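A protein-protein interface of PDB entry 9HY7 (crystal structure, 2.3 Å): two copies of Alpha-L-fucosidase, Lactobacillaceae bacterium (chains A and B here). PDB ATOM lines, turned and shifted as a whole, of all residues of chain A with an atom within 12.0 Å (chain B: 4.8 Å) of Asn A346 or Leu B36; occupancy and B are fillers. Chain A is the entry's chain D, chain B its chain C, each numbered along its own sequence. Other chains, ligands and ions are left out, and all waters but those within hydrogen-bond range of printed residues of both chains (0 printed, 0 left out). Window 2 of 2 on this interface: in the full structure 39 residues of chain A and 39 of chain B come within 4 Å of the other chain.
Among the printed residues, pairs that only touch across the chains: Asn A346 with Leu B36 (3.4 Å), Tyr A400 with Ile B37 (3.5 Å), Tyr A400 with Thr B34 (3.6 Å), Val A349 with Ile B37 (3.7 Å), Val A344 with Ile B37 (3.9 Å) and Val A349 with Trp B33 (3.97 Å).
Asn A346 touches just one residue of chain B: Leu B36. Of chain A, only Val A349 and Tyr A400 come within 4 Å of Trp B33. Printed residues of chain A within 4 Å of Thr B34: Tyr A400 (3.6 Å). No residue of chain A comes within 4 Å of Glu B35. His B38 touches one residue of chain A. His B39 touches none of the printed residues of chain A. Printed residues of chain B within 4 Å of Val A344: Ile B37 (3.9 Å). Of the printed residues of chain A, Ile B37 touches Val A344 (3.9 Å), Val A349 (3.7 Å) and Tyr A400 (3.5 Å). Of the printed residues of chain B, Val A349 touches Trp B33 and Ile B37. Printed residues of chain B within 4 Å of Tyr A400: Trp B33, Thr B34, Ile B37 and His B38. Gly A401 touches none of the printed residues of chain B. The nearest residue of chain A that does not touch Leu B36 is Val A349 (4.9 Å). The nearest printed residue of chain A that does not touch Ile B37 is Gly A345 (4.02 Å).
Of the 20 printed residues of chain A, 4 touch a printed residue of chain B. Printed residues of chain A that touch a printed residue of chain B: Val A344, Asn A346, Val A349 and Tyr A400. Hydrophobic or aromatic side chains of chain A that line the printed part of chain B: Val A349 and Tyr A400. Of the 9 printed residues of chain B, 5 touch a printed residue of chain A. Among the printed residues, 8 pairs touch across the chains. Among the printed residues, no Asp or Glu carboxylate lies within 4 Å of a Lys or Arg side-chain nitrogen of the other chain.
No position is printed for both chains. Of the 8 pairs that touch across the chains among the printed residues, none has its exchanged pair printed and touching as well.
The backbone NH (N) of Val A349 sits at hydrogen-bond distance from the side-chain amide oxygen (OD1) of Asn A346, at 2.7 Å. The side-chain amide oxygen of Asn A346 lies within hydrogen-bond range of the backbone NH of Asn A348, at 2.7 Å. The backbone carbonyl oxygen (O) of Tyr A398 lies within hydrogen-bond range of the backbone NH (N) of Val A344 (2.8 Å). A ring nitrogen (ND1) of His B38 is in hydrogen-bond range of the side-chain hydroxyl (OG1) of Thr B34 (2.6 Å).
O of Tyr A400 sits at hydrogen-bond distance from NE2 of His B38 (2.8 Å). N of Trp B33 lies within hydrogen-bond range of OH of Tyr A400 (2.9 Å).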
ATOM      1  N   GLN A 342     -29.411  25.749  -9.350  1.00  0.00           N
ATOM      2  CA  GLN A 342     -28.416  25.048 -10.140  1.00  0.00           C
ATOM      3  C   GLN A 342     -28.988  24.577 -11.469  1.00  0.00           C
ATOM      4  O   GLN A 342     -30.196  24.590 -11.655  1.00  0.00           O
ATOM      5  CB  GLN A 342     -27.822  23.970  -9.252  1.00  0.00           C
ATOM      6  CG  GLN A 342     -26.959  24.565  -8.146  1.00  0.00           C
ATOM      7  CD  GLN A 342     -26.482  23.497  -7.196  1.00  0.00           C
ATOM      8  OE1 GLN A 342     -27.235  22.896  -6.416  1.00  0.00           O
ATOM      9  NE2 GLN A 342     -25.205  23.207  -7.327  1.00  0.00           N
ATOM     10  N   VAL A 343     -28.095  24.176 -12.385  1.00  0.00           N
ATOM     11  CA  VAL A 343     -28.436  23.639 -13.688  1.00  0.00           C
ATOM     12  C   VAL A 343     -28.940  22.196 -13.538  1.00  0.00           C
ATOM     13  O   VAL A 343     -28.509  21.449 -12.647  1.00  0.00           O
ATOM     14  CB  VAL A 343     -27.214  23.757 -14.628  1.00  0.00           C
ATOM     15  CG1 VAL A 343     -27.532  23.286 -16.044  1.00  0.00           C
ATOM     16  CG2 VAL A 343     -26.687  25.192 -14.679  1.00  0.00           C
ATOM     17  N   VAL A 344     -29.894  21.824 -14.406  1.00  0.00           N
ATOM     18  CA  VAL A 344     -30.468  20.481 -14.407  1.00  0.00           C
ATOM     19  C   VAL A 344     -29.763  19.623 -15.458  1.00  0.00           C
ATOM     20  O   VAL A 344     -29.831  19.931 -16.652  1.00  0.00           O
ATOM     21  CB  VAL A 344     -31.988  20.558 -14.695  1.00  0.00           C
ATOM     22  CG1 VAL A 344     -32.616  19.180 -14.981  1.00  0.00           C
ATOM     23  CG2 VAL A 344     -32.748  21.316 -13.584  1.00  0.00           C
ATOM     24  N   GLY A 345     -29.207  18.523 -15.033  1.00  0.00           N
ATOM     25  CA  GLY A 345     -28.640  17.580 -15.931  1.00  0.00           C
ATOM     26  C   GLY A 345     -29.620  16.437 -16.013  1.00  0.00           C
ATOM     27  O   GLY A 345     -30.711  16.608 -16.469  1.00  0.00           O
ATOM     28  N   ASN A 346     -29.213  15.277 -15.540  1.00  0.00           N
ATOM     29  CA  ASN A 346     -30.061  14.094 -15.474  1.00  0.00           C
ATOM     30  C   ASN A 346     -29.580  13.121 -14.400  1.00  0.00           C
ATOM     31  O   ASN A 346     -28.754  13.460 -13.607  1.00  0.00           O
ATOM     32  CB  ASN A 346     -30.280  13.430 -16.828  1.00  0.00           C
ATOM     33  CG  ASN A 346     -29.080  12.710 -17.320  1.00  0.00           C
ATOM     34  OD1 ASN A 346     -28.219  12.302 -16.563  1.00  0.00           O
ATOM     35  ND2 ASN A 346     -29.019  12.542 -18.601  1.00  0.00           N
ATOM     36  N   ASP A 347     -30.138  11.923 -14.350  1.00  0.00           N
ATOM     37  CA  ASP A 347     -29.684  10.946 -13.372  1.00  0.00           C
ATOM     38  C   ASP A 347     -28.243  10.559 -13.575  1.00  0.00           C
ATOM     39  O   ASP A 347     -27.526  10.357 -12.618  1.00  0.00           O
ATOM     40  CB  ASP A 347     -30.527   9.688 -13.417  1.00  0.00           C
ATOM     41  CG  ASP A 347     -31.951   9.918 -12.997  1.00  0.00           C
ATOM     42  OD1 ASP A 347     -32.540  10.937 -13.426  1.00  0.00           O
ATOM     43  OD2 ASP A 347     -32.486   9.059 -12.270  1.00  0.00           O
ATOM     44  N   ASN A 348     -27.821  10.353 -14.807  1.00  0.00           N
ATOM     45  CA  ASN A 348     -26.437  10.051 -15.020  1.00  0.00           C
ATOM     46  C   ASN A 348     -25.487  11.206 -14.811  1.00  0.00           C
ATOM     47  O   ASN A 348     -24.464  11.033 -14.223  1.00  0.00           O
ATOM     48  CB  ASN A 348     -26.227   9.400 -16.368  1.00  0.00           C
ATOM     49  CG  ASN A 348     -26.930   8.076 -16.472  1.00  0.00           C
ATOM     50  OD1 ASN A 348     -27.708   7.850 -17.384  1.00  0.00           O
ATOM     51  ND2 ASN A 348     -26.675   7.198 -15.522  1.00  0.00           N
ATOM     52  N   VAL A 349     -25.811  12.385 -15.306  1.00  0.00           N
ATOM     53  CA  VAL A 349     -24.916  13.520 -15.115  1.00  0.00           C
ATOM     54  C   VAL A 349     -25.622  14.500 -14.207  1.00  0.00           C
ATOM     55  O   VAL A 349     -26.488  15.203 -14.615  1.00  0.00           O
ATOM     56  CB  VAL A 349     -24.429  14.097 -16.450  1.00  0.00           C
ATOM     57  CG1 VAL A 349     -25.574  14.424 -17.368  1.00  0.00           C
ATOM     58  CG2 VAL A 349     -23.503  15.256 -16.232  1.00  0.00           C
ATOM     59  N   VAL A 350     -25.138  14.583 -12.991  1.00  0.00           N
ATOM     60  CA  VAL A 350     -25.788  15.314 -11.915  1.00  0.00           C
ATOM     61  C   VAL A 350     -25.147  16.696 -11.817  1.00  0.00           C
ATOM     62  O   VAL A 350     -23.957  16.817 -11.523  1.00  0.00           O
ATOM     63  CB  VAL A 350     -25.777  14.546 -10.570  1.00  0.00           C
ATOM     64  CG1 VAL A 350     -26.181  15.417  -9.364  1.00  0.00           C
ATOM     65  CG2 VAL A 350     -26.622  13.270 -10.622  1.00  0.00           C
ATOM     66  N   LEU A 351     -25.947  17.747 -12.049  1.00  0.00           N
ATOM     67  CA  LEU A 351     -25.406  19.104 -12.062  1.00  0.00           C
ATOM     68  C   LEU A 351     -25.844  19.887 -10.813  1.00  0.00           C
ATOM     69  O   LEU A 351     -25.242  20.915 -10.502  1.00  0.00           O
ATOM     70  CB  LEU A 351     -25.727  19.815 -13.378  1.00  0.00           C
ATOM     71  CG  LEU A 351     -25.117  19.186 -14.640  1.00  0.00           C
ATOM     72  CD1 LEU A 351     -25.703  19.811 -15.894  1.00  0.00           C
ATOM     73  CD2 LEU A 351     -23.576  19.247 -14.663  1.00  0.00           C
ATOM     74  N   GLY A 352     -26.898  19.417 -10.110  1.00  0.00           N
ATOM     75  CA  GLY A 352     -27.276  19.933  -8.797  1.00  0.00           C
ATOM     76  C   GLY A 352     -28.755  20.342  -8.712  1.00  0.00           C
ATOM     77  O   GLY A 352     -29.325  20.324  -7.626  1.00  0.00           O
ATOM     78  N   GLY A 353     -29.381  20.697  -9.852  1.00  0.00           N
ATOM     79  CA  GLY A 353     -30.714  21.291  -9.858  1.00  0.00           C
ATOM     80  C   GLY A 353     -31.860  20.280 -10.034  1.00  0.00           C
ATOM     81  O   GLY A 353     -33.012  20.719 -10.127  1.00  0.00           O
ATOM     82  N   GLU A 354     -31.557  18.961 -10.007  1.00  0.00           N
ATOM     83  CA  GLU A 354     -32.487  17.935 -10.476  1.00  0.00           C
ATOM     84  C   GLU A 354     -33.655  17.728  -9.500  1.00  0.00           C
ATOM     85  O   GLU A 354     -34.793  17.564  -9.945  1.00  0.00           O
ATOM     86  CB  GLU A 354     -31.859  16.557 -10.754  1.00  0.00           C
ATOM     87  CG  GLU A 354     -30.806  16.539 -11.855  1.00  0.00           C
ATOM     88  CD  GLU A 354     -29.444  17.166 -11.530  1.00  0.00           C
ATOM     89  OE1 GLU A 354     -29.107  17.373 -10.336  1.00  0.00           O
ATOM     90  OE2 GLU A 354     -28.721  17.499 -12.502  1.00  0.00           O
ATOM     91  N   GLY A 355     -33.377  17.680  -8.182  1.00  0.00           N
ATOM     92  CA  GLY A 355     -34.411  17.295  -7.230  1.00  0.00           C
ATOM     93  C   GLY A 355     -35.482  18.375  -7.101  1.00  0.00           C
ATOM     94  O   GLY A 355     -35.262  19.528  -7.453  1.00  0.00           O
ATOM     95  N   VAL A 356     -36.648  17.999  -6.571  1.00  0.00           N
ATOM     96  CA  VAL A 356     -37.647  18.963  -6.150  1.00  0.00           C
ATOM     97  C   VAL A 356     -37.023  19.937  -5.141  1.00  0.00           C
ATOM     98  O   VAL A 356     -36.238  19.546  -4.261  1.00  0.00           O
ATOM     99  CB  VAL A 356     -38.835  18.163  -5.581  1.00  0.00           C
ATOM    100  CG1 VAL A 356     -39.855  19.058  -4.910  1.00  0.00           C
ATOM    101  CG2 VAL A 356     -39.498  17.305  -6.684  1.00  0.00           C
ATOM    102  N   GLY A 397     -34.620  23.873 -11.438  1.00  0.00           N
ATOM    103  CA  GLY A 397     -33.317  24.418 -11.788  1.00  0.00           C
ATOM    104  C   GLY A 397     -33.279  24.857 -13.254  1.00  0.00           C
ATOM    105  O   GLY A 397     -34.241  24.641 -14.014  1.00  0.00           O
ATOM    106  N   TYR A 398     -32.159  25.460 -13.661  1.00  0.00           N
ATOM    107  CA  TYR A 398     -32.032  25.983 -15.010  1.00  0.00           C
ATOM    108  C   TYR A 398     -31.998  24.830 -16.014  1.00  0.00           C
ATOM    109  O   TYR A 398     -31.340  23.818 -15.762  1.00  0.00           O
ATOM    110  CB  TYR A 398     -30.717  26.753 -15.135  1.00  0.00           C
ATOM    111  CG  TYR A 398     -30.658  27.922 -14.162  1.00  0.00           C
ATOM    112  CD1 TYR A 398     -31.530  28.987 -14.323  1.00  0.00           C
ATOM    113  CD2 TYR A 398     -29.729  27.978 -13.130  1.00  0.00           C
ATOM    114  CE1 TYR A 398     -31.510  30.066 -13.460  1.00  0.00           C
ATOM    115  CE2 TYR A 398     -29.688  29.054 -12.258  1.00  0.00           C
ATOM    116  CZ  TYR A 398     -30.586  30.084 -12.431  1.00  0.00           C
ATOM    117  OH  TYR A 398     -30.637  31.177 -11.628  1.00  0.00           O
ATOM    118  N   PRO A 399     -32.621  24.983 -17.204  1.00  0.00           N
ATOM    119  CA  PRO A 399     -32.353  24.074 -18.313  1.00  0.00           C
ATOM    120  C   PRO A 399     -30.858  24.084 -18.618  1.00  0.00           C
ATOM    121  O   PRO A 399     -30.227  25.155 -18.568  1.00  0.00           O
ATOM    122  CB  PRO A 399     -33.130  24.653 -19.514  1.00  0.00           C
ATOM    123  CG  PRO A 399     -34.102  25.633 -18.915  1.00  0.00           C
ATOM    124  CD  PRO A 399     -33.519  26.093 -17.562  1.00  0.00           C
ATOM    125  N   TYR A 400     -30.300  22.888 -18.868  1.00  0.00           N
ATOM    126  CA  TYR A 400     -28.914  22.796 -19.296  1.00  0.00           C
ATOM    127  C   TYR A 400     -28.658  23.840 -20.388  1.00  0.00           C
ATOM    128  O   TYR A 400     -29.495  24.028 -21.275  1.00  0.00           O
ATOM    129  CB  TYR A 400     -28.614  21.379 -19.783  1.00  0.00           C
ATOM    130  CG  TYR A 400     -27.171  21.273 -20.250  1.00  0.00           C
ATOM    131  CD1 TYR A 400     -26.108  21.222 -19.335  1.00  0.00           C
ATOM    132  CD2 TYR A 400     -26.876  21.229 -21.618  1.00  0.00           C
ATOM    133  CE1 TYR A 400     -24.799  21.179 -19.773  1.00  0.00           C
ATOM    134  CE2 TYR A 400     -25.565  21.174 -22.064  1.00  0.00           C
ATOM    135  CZ  TYR A 400     -24.533  21.141 -21.135  1.00  0.00           C
ATOM    136  OH  TYR A 400     -23.251  21.058 -21.571  1.00  0.00           O
ATOM    137  N   GLY A 401     -27.517  24.537 -20.307  1.00  0.00           N
ATOM    138  CA  GLY A 401     -27.194  25.542 -21.312  1.00  0.00           C
ATOM    139  C   GLY A 401     -27.560  26.958 -20.866  1.00  0.00           C
ATOM    140  O   GLY A 401     -27.212  27.931 -21.542  1.00  0.00           O
ATOM    141  N   TRP B  33     -23.163  19.390 -23.971  1.00  0.00           N
ATOM    142  CA  TRP B  33     -23.878  18.137 -23.735  1.00  0.00           C
ATOM    143  C   TRP B  33     -25.310  18.185 -24.275  1.00  0.00           C
ATOM    144  O   TRP B  33     -26.092  17.286 -23.976  1.00  0.00           O
ATOM    145  CB  TRP B  33     -23.880  17.777 -22.245  1.00  0.00           C
ATOM    146  CG  TRP B  33     -22.644  17.099 -21.703  1.00  0.00           C
ATOM    147  CD1 TRP B  33     -21.397  17.637 -21.572  1.00  0.00           C
ATOM    148  CD2 TRP B  33     -22.573  15.769 -21.132  1.00  0.00           C
ATOM    149  NE1 TRP B  33     -20.537  16.721 -20.997  1.00  0.00           N
ATOM    150  CE2 TRP B  33     -21.236  15.570 -20.709  1.00  0.00           C
ATOM    151  CE3 TRP B  33     -23.500  14.734 -20.941  1.00  0.00           C
ATOM    152  CZ2 TRP B  33     -20.809  14.378 -20.102  1.00  0.00           C
ATOM    153  CZ3 TRP B  33     -23.082  13.559 -20.331  1.00  0.00           C
ATOM    154  CH2 TRP B  33     -21.748  13.392 -19.907  1.00  0.00           C
ATOM    155  N   THR B  34     -25.658  19.173 -25.103  1.00  0.00           N
ATOM    156  CA  THR B  34     -27.054  19.401 -25.482  1.00  0.00           C
ATOM    157  C   THR B  34     -27.712  18.141 -26.067  1.00  0.00           C
ATOM    158  O   THR B  34     -28.863  17.827 -25.740  1.00  0.00           O
ATOM    159  CB  THR B  34     -27.190  20.619 -26.392  1.00  0.00           C
ATOM    160  OG1 THR B  34     -28.582  20.777 -26.627  1.00  0.00           O
ATOM    161  CG2 THR B  34     -26.463  20.498 -27.726  1.00  0.00           C
ATOM    162  N   GLU B  35     -26.996  17.405 -26.932  1.00  0.00           N
ATOM    163  CA  GLU B  35     -27.604  16.252 -27.594  1.00  0.00           C
ATOM    164  C   GLU B  35     -28.174  15.261 -26.570  1.00  0.00           C
ATOM    165  O   GLU B  35     -29.320  14.828 -26.699  1.00  0.00           O
ATOM    166  CB  GLU B  35     -26.713  15.537 -28.615  1.00  0.00           C
ATOM    167  CG  GLU B  35     -27.446  14.407 -29.336  1.00  0.00           C
ATOM    168  CD  GLU B  35     -26.526  13.624 -30.293  1.00  0.00           C
ATOM    169  OE1 GLU B  35     -25.266  13.629 -30.160  1.00  0.00           O
ATOM    170  OE2 GLU B  35     -27.083  13.011 -31.222  1.00  0.00           O
ATOM    171  N   LEU B  36     -27.380  14.902 -25.558  1.00  0.00           N
ATOM    172  CA  LEU B  36     -27.827  13.933 -24.564  1.00  0.00           C
ATOM    173  C   LEU B  36     -28.782  14.590 -23.548  1.00  0.00           C
ATOM    174  O   LEU B  36     -29.889  14.081 -23.311  1.00  0.00           O
ATOM    175  CB  LEU B  36     -26.622  13.272 -23.908  1.00  0.00           C
ATOM    176  CG  LEU B  36     -26.934  12.096 -22.974  1.00  0.00           C
ATOM    177  CD1 LEU B  36     -25.700  11.245 -22.763  1.00  0.00           C
ATOM    178  CD2 LEU B  36     -27.352  12.564 -21.596  1.00  0.00           C
ATOM    179  N   ILE B  37     -28.373  15.725 -22.940  1.00  0.00           N
ATOM    180  CA  ILE B  37     -29.118  16.257 -21.805  1.00  0.00           C
ATOM    181  C   ILE B  37     -30.484  16.803 -22.238  1.00  0.00           C
ATOM    182  O   ILE B  37     -31.448  16.695 -21.472  1.00  0.00           O
ATOM    183  CB  ILE B  37     -28.290  17.268 -20.981  1.00  0.00           C
ATOM    184  CG1 ILE B  37     -27.099  16.540 -20.356  1.00  0.00           C
ATOM    185  CG2 ILE B  37     -29.161  17.955 -19.920  1.00  0.00           C
ATOM    186  CD1 ILE B  37     -26.146  17.401 -19.568  1.00  0.00           C
ATOM    187  N   HIS B  38     -30.591  17.361 -23.451  1.00  0.00           N
ATOM    188  CA  HIS B  38     -31.882  17.832 -23.909  1.00  0.00           C
ATOM    189  C   HIS B  38     -32.662  16.739 -24.660  1.00  0.00           C
ATOM    190  O   HIS B  38     -33.668  17.062 -25.298  1.00  0.00           O
ATOM    191  CB  HIS B  38     -31.717  19.076 -24.787  1.00  0.00           C
ATOM    192  CG  HIS B  38     -31.197  20.275 -24.054  1.00  0.00           C
ATOM    193  ND1 HIS B  38     -30.112  21.016 -24.488  1.00  0.00           N
ATOM    194  CD2 HIS B  38     -31.640  20.865 -22.923  1.00  0.00           C
ATOM    195  CE1 HIS B  38     -29.910  22.021 -23.644  1.00  0.00           C
ATOM    196  NE2 HIS B  38     -30.837  21.961 -22.704  1.00  0.00           N
ATOM    197  N   HIS B  39     -32.185  15.475 -24.632  1.00  0.00           N
ATOM    198  CA  HIS B  39     -32.873  14.327 -25.239  1.00  0.00           C
ATOM    199  C   HIS B  39     -33.231  14.590 -26.695  1.00  0.00           C
ATOM    200  O   HIS B  39     -34.363  14.364 -27.072  1.00  0.00           O
ATOM    201  CB  HIS B  39     -34.198  13.974 -24.530  1.00  0.00           C
ATOM    202  CG  HIS B  39     -34.062  13.874 -23.043  1.00  0.00           C
ATOM    203  ND1 HIS B  39     -34.677  14.793 -22.212  1.00  0.00           N
ATOM    204  CD2 HIS B  39     -33.384  13.017 -22.238  1.00  0.00           C
ATOM    205  CE1 HIS B  39     -34.377  14.505 -20.948  1.00  0.00           C
ATOM    206  NE2 HIS B  39     -33.558  13.460 -20.949  1.00  0.00           N
ATOM    207  N   TYR B 128     -15.883   8.590 -24.542  1.00  0.00           N
ATOM    208  CA  TYR B 128     -17.302   8.304 -24.475  1.00  0.00           C
ATOM    209  C   TYR B 128     -17.986   8.961 -25.670  1.00  0.00           C
ATOM    210  O   TYR B 128     -17.984  10.184 -25.754  1.00  0.00           O
ATOM    211  CB  TYR B 128     -17.770   8.870 -23.122  1.00  0.00           C
ATOM    212  CG  TYR B 128     -19.264   8.860 -22.807  1.00  0.00           C
ATOM    213  CD1 TYR B 128     -20.117   7.864 -23.280  1.00  0.00           C
ATOM    214  CD2 TYR B 128     -19.821   9.845 -21.999  1.00  0.00           C
ATOM    215  CE1 TYR B 128     -21.474   7.845 -22.964  1.00  0.00           C
ATOM    216  CE2 TYR B 128     -21.174   9.848 -21.670  1.00  0.00           C
ATOM    217  CZ  TYR B 128     -21.998   8.836 -22.141  1.00  0.00           C
ATOM    218  OH  TYR B 128     -23.314   8.834 -21.812  1.00  0.00           O
ATOM    219  N   TRP B 130     -21.287   9.320 -28.494  1.00  0.00           N
ATOM    220  CA  TRP B 130     -22.736   9.196 -28.651  1.00  0.00           C
ATOM    221  C   TRP B 130     -23.100   8.933 -30.112  1.00  0.00           C
ATOM    222  O   TRP B 130     -24.267   8.731 -30.427  1.00  0.00           O
ATOM    223  CB  TRP B 130     -23.470  10.476 -28.198  1.00  0.00           C
ATOM    224  CG  TRP B 130     -23.195  10.912 -26.780  1.00  0.00           C
ATOM    225  CD1 TRP B 130     -22.801  10.127 -25.727  1.00  0.00           C
ATOM    226  CD2 TRP B 130     -23.264  12.268 -26.271  1.00  0.00           C
ATOM    227  NE1 TRP B 130     -22.613  10.895 -24.602  1.00  0.00           N
ATOM    228  CE2 TRP B 130     -22.888  12.212 -24.907  1.00  0.00           C
ATOM    229  CE3 TRP B 130     -23.595  13.505 -26.832  1.00  0.00           C
ATOM    230  CZ2 TRP B 130     -22.861  13.354 -24.107  1.00  0.00           C
ATOM    231  CZ3 TRP B 130     -23.551  14.627 -26.031  1.00  0.00           C
ATOM    232  CH2 TRP B 130     -23.196  14.563 -24.685  1.00  0.00           C
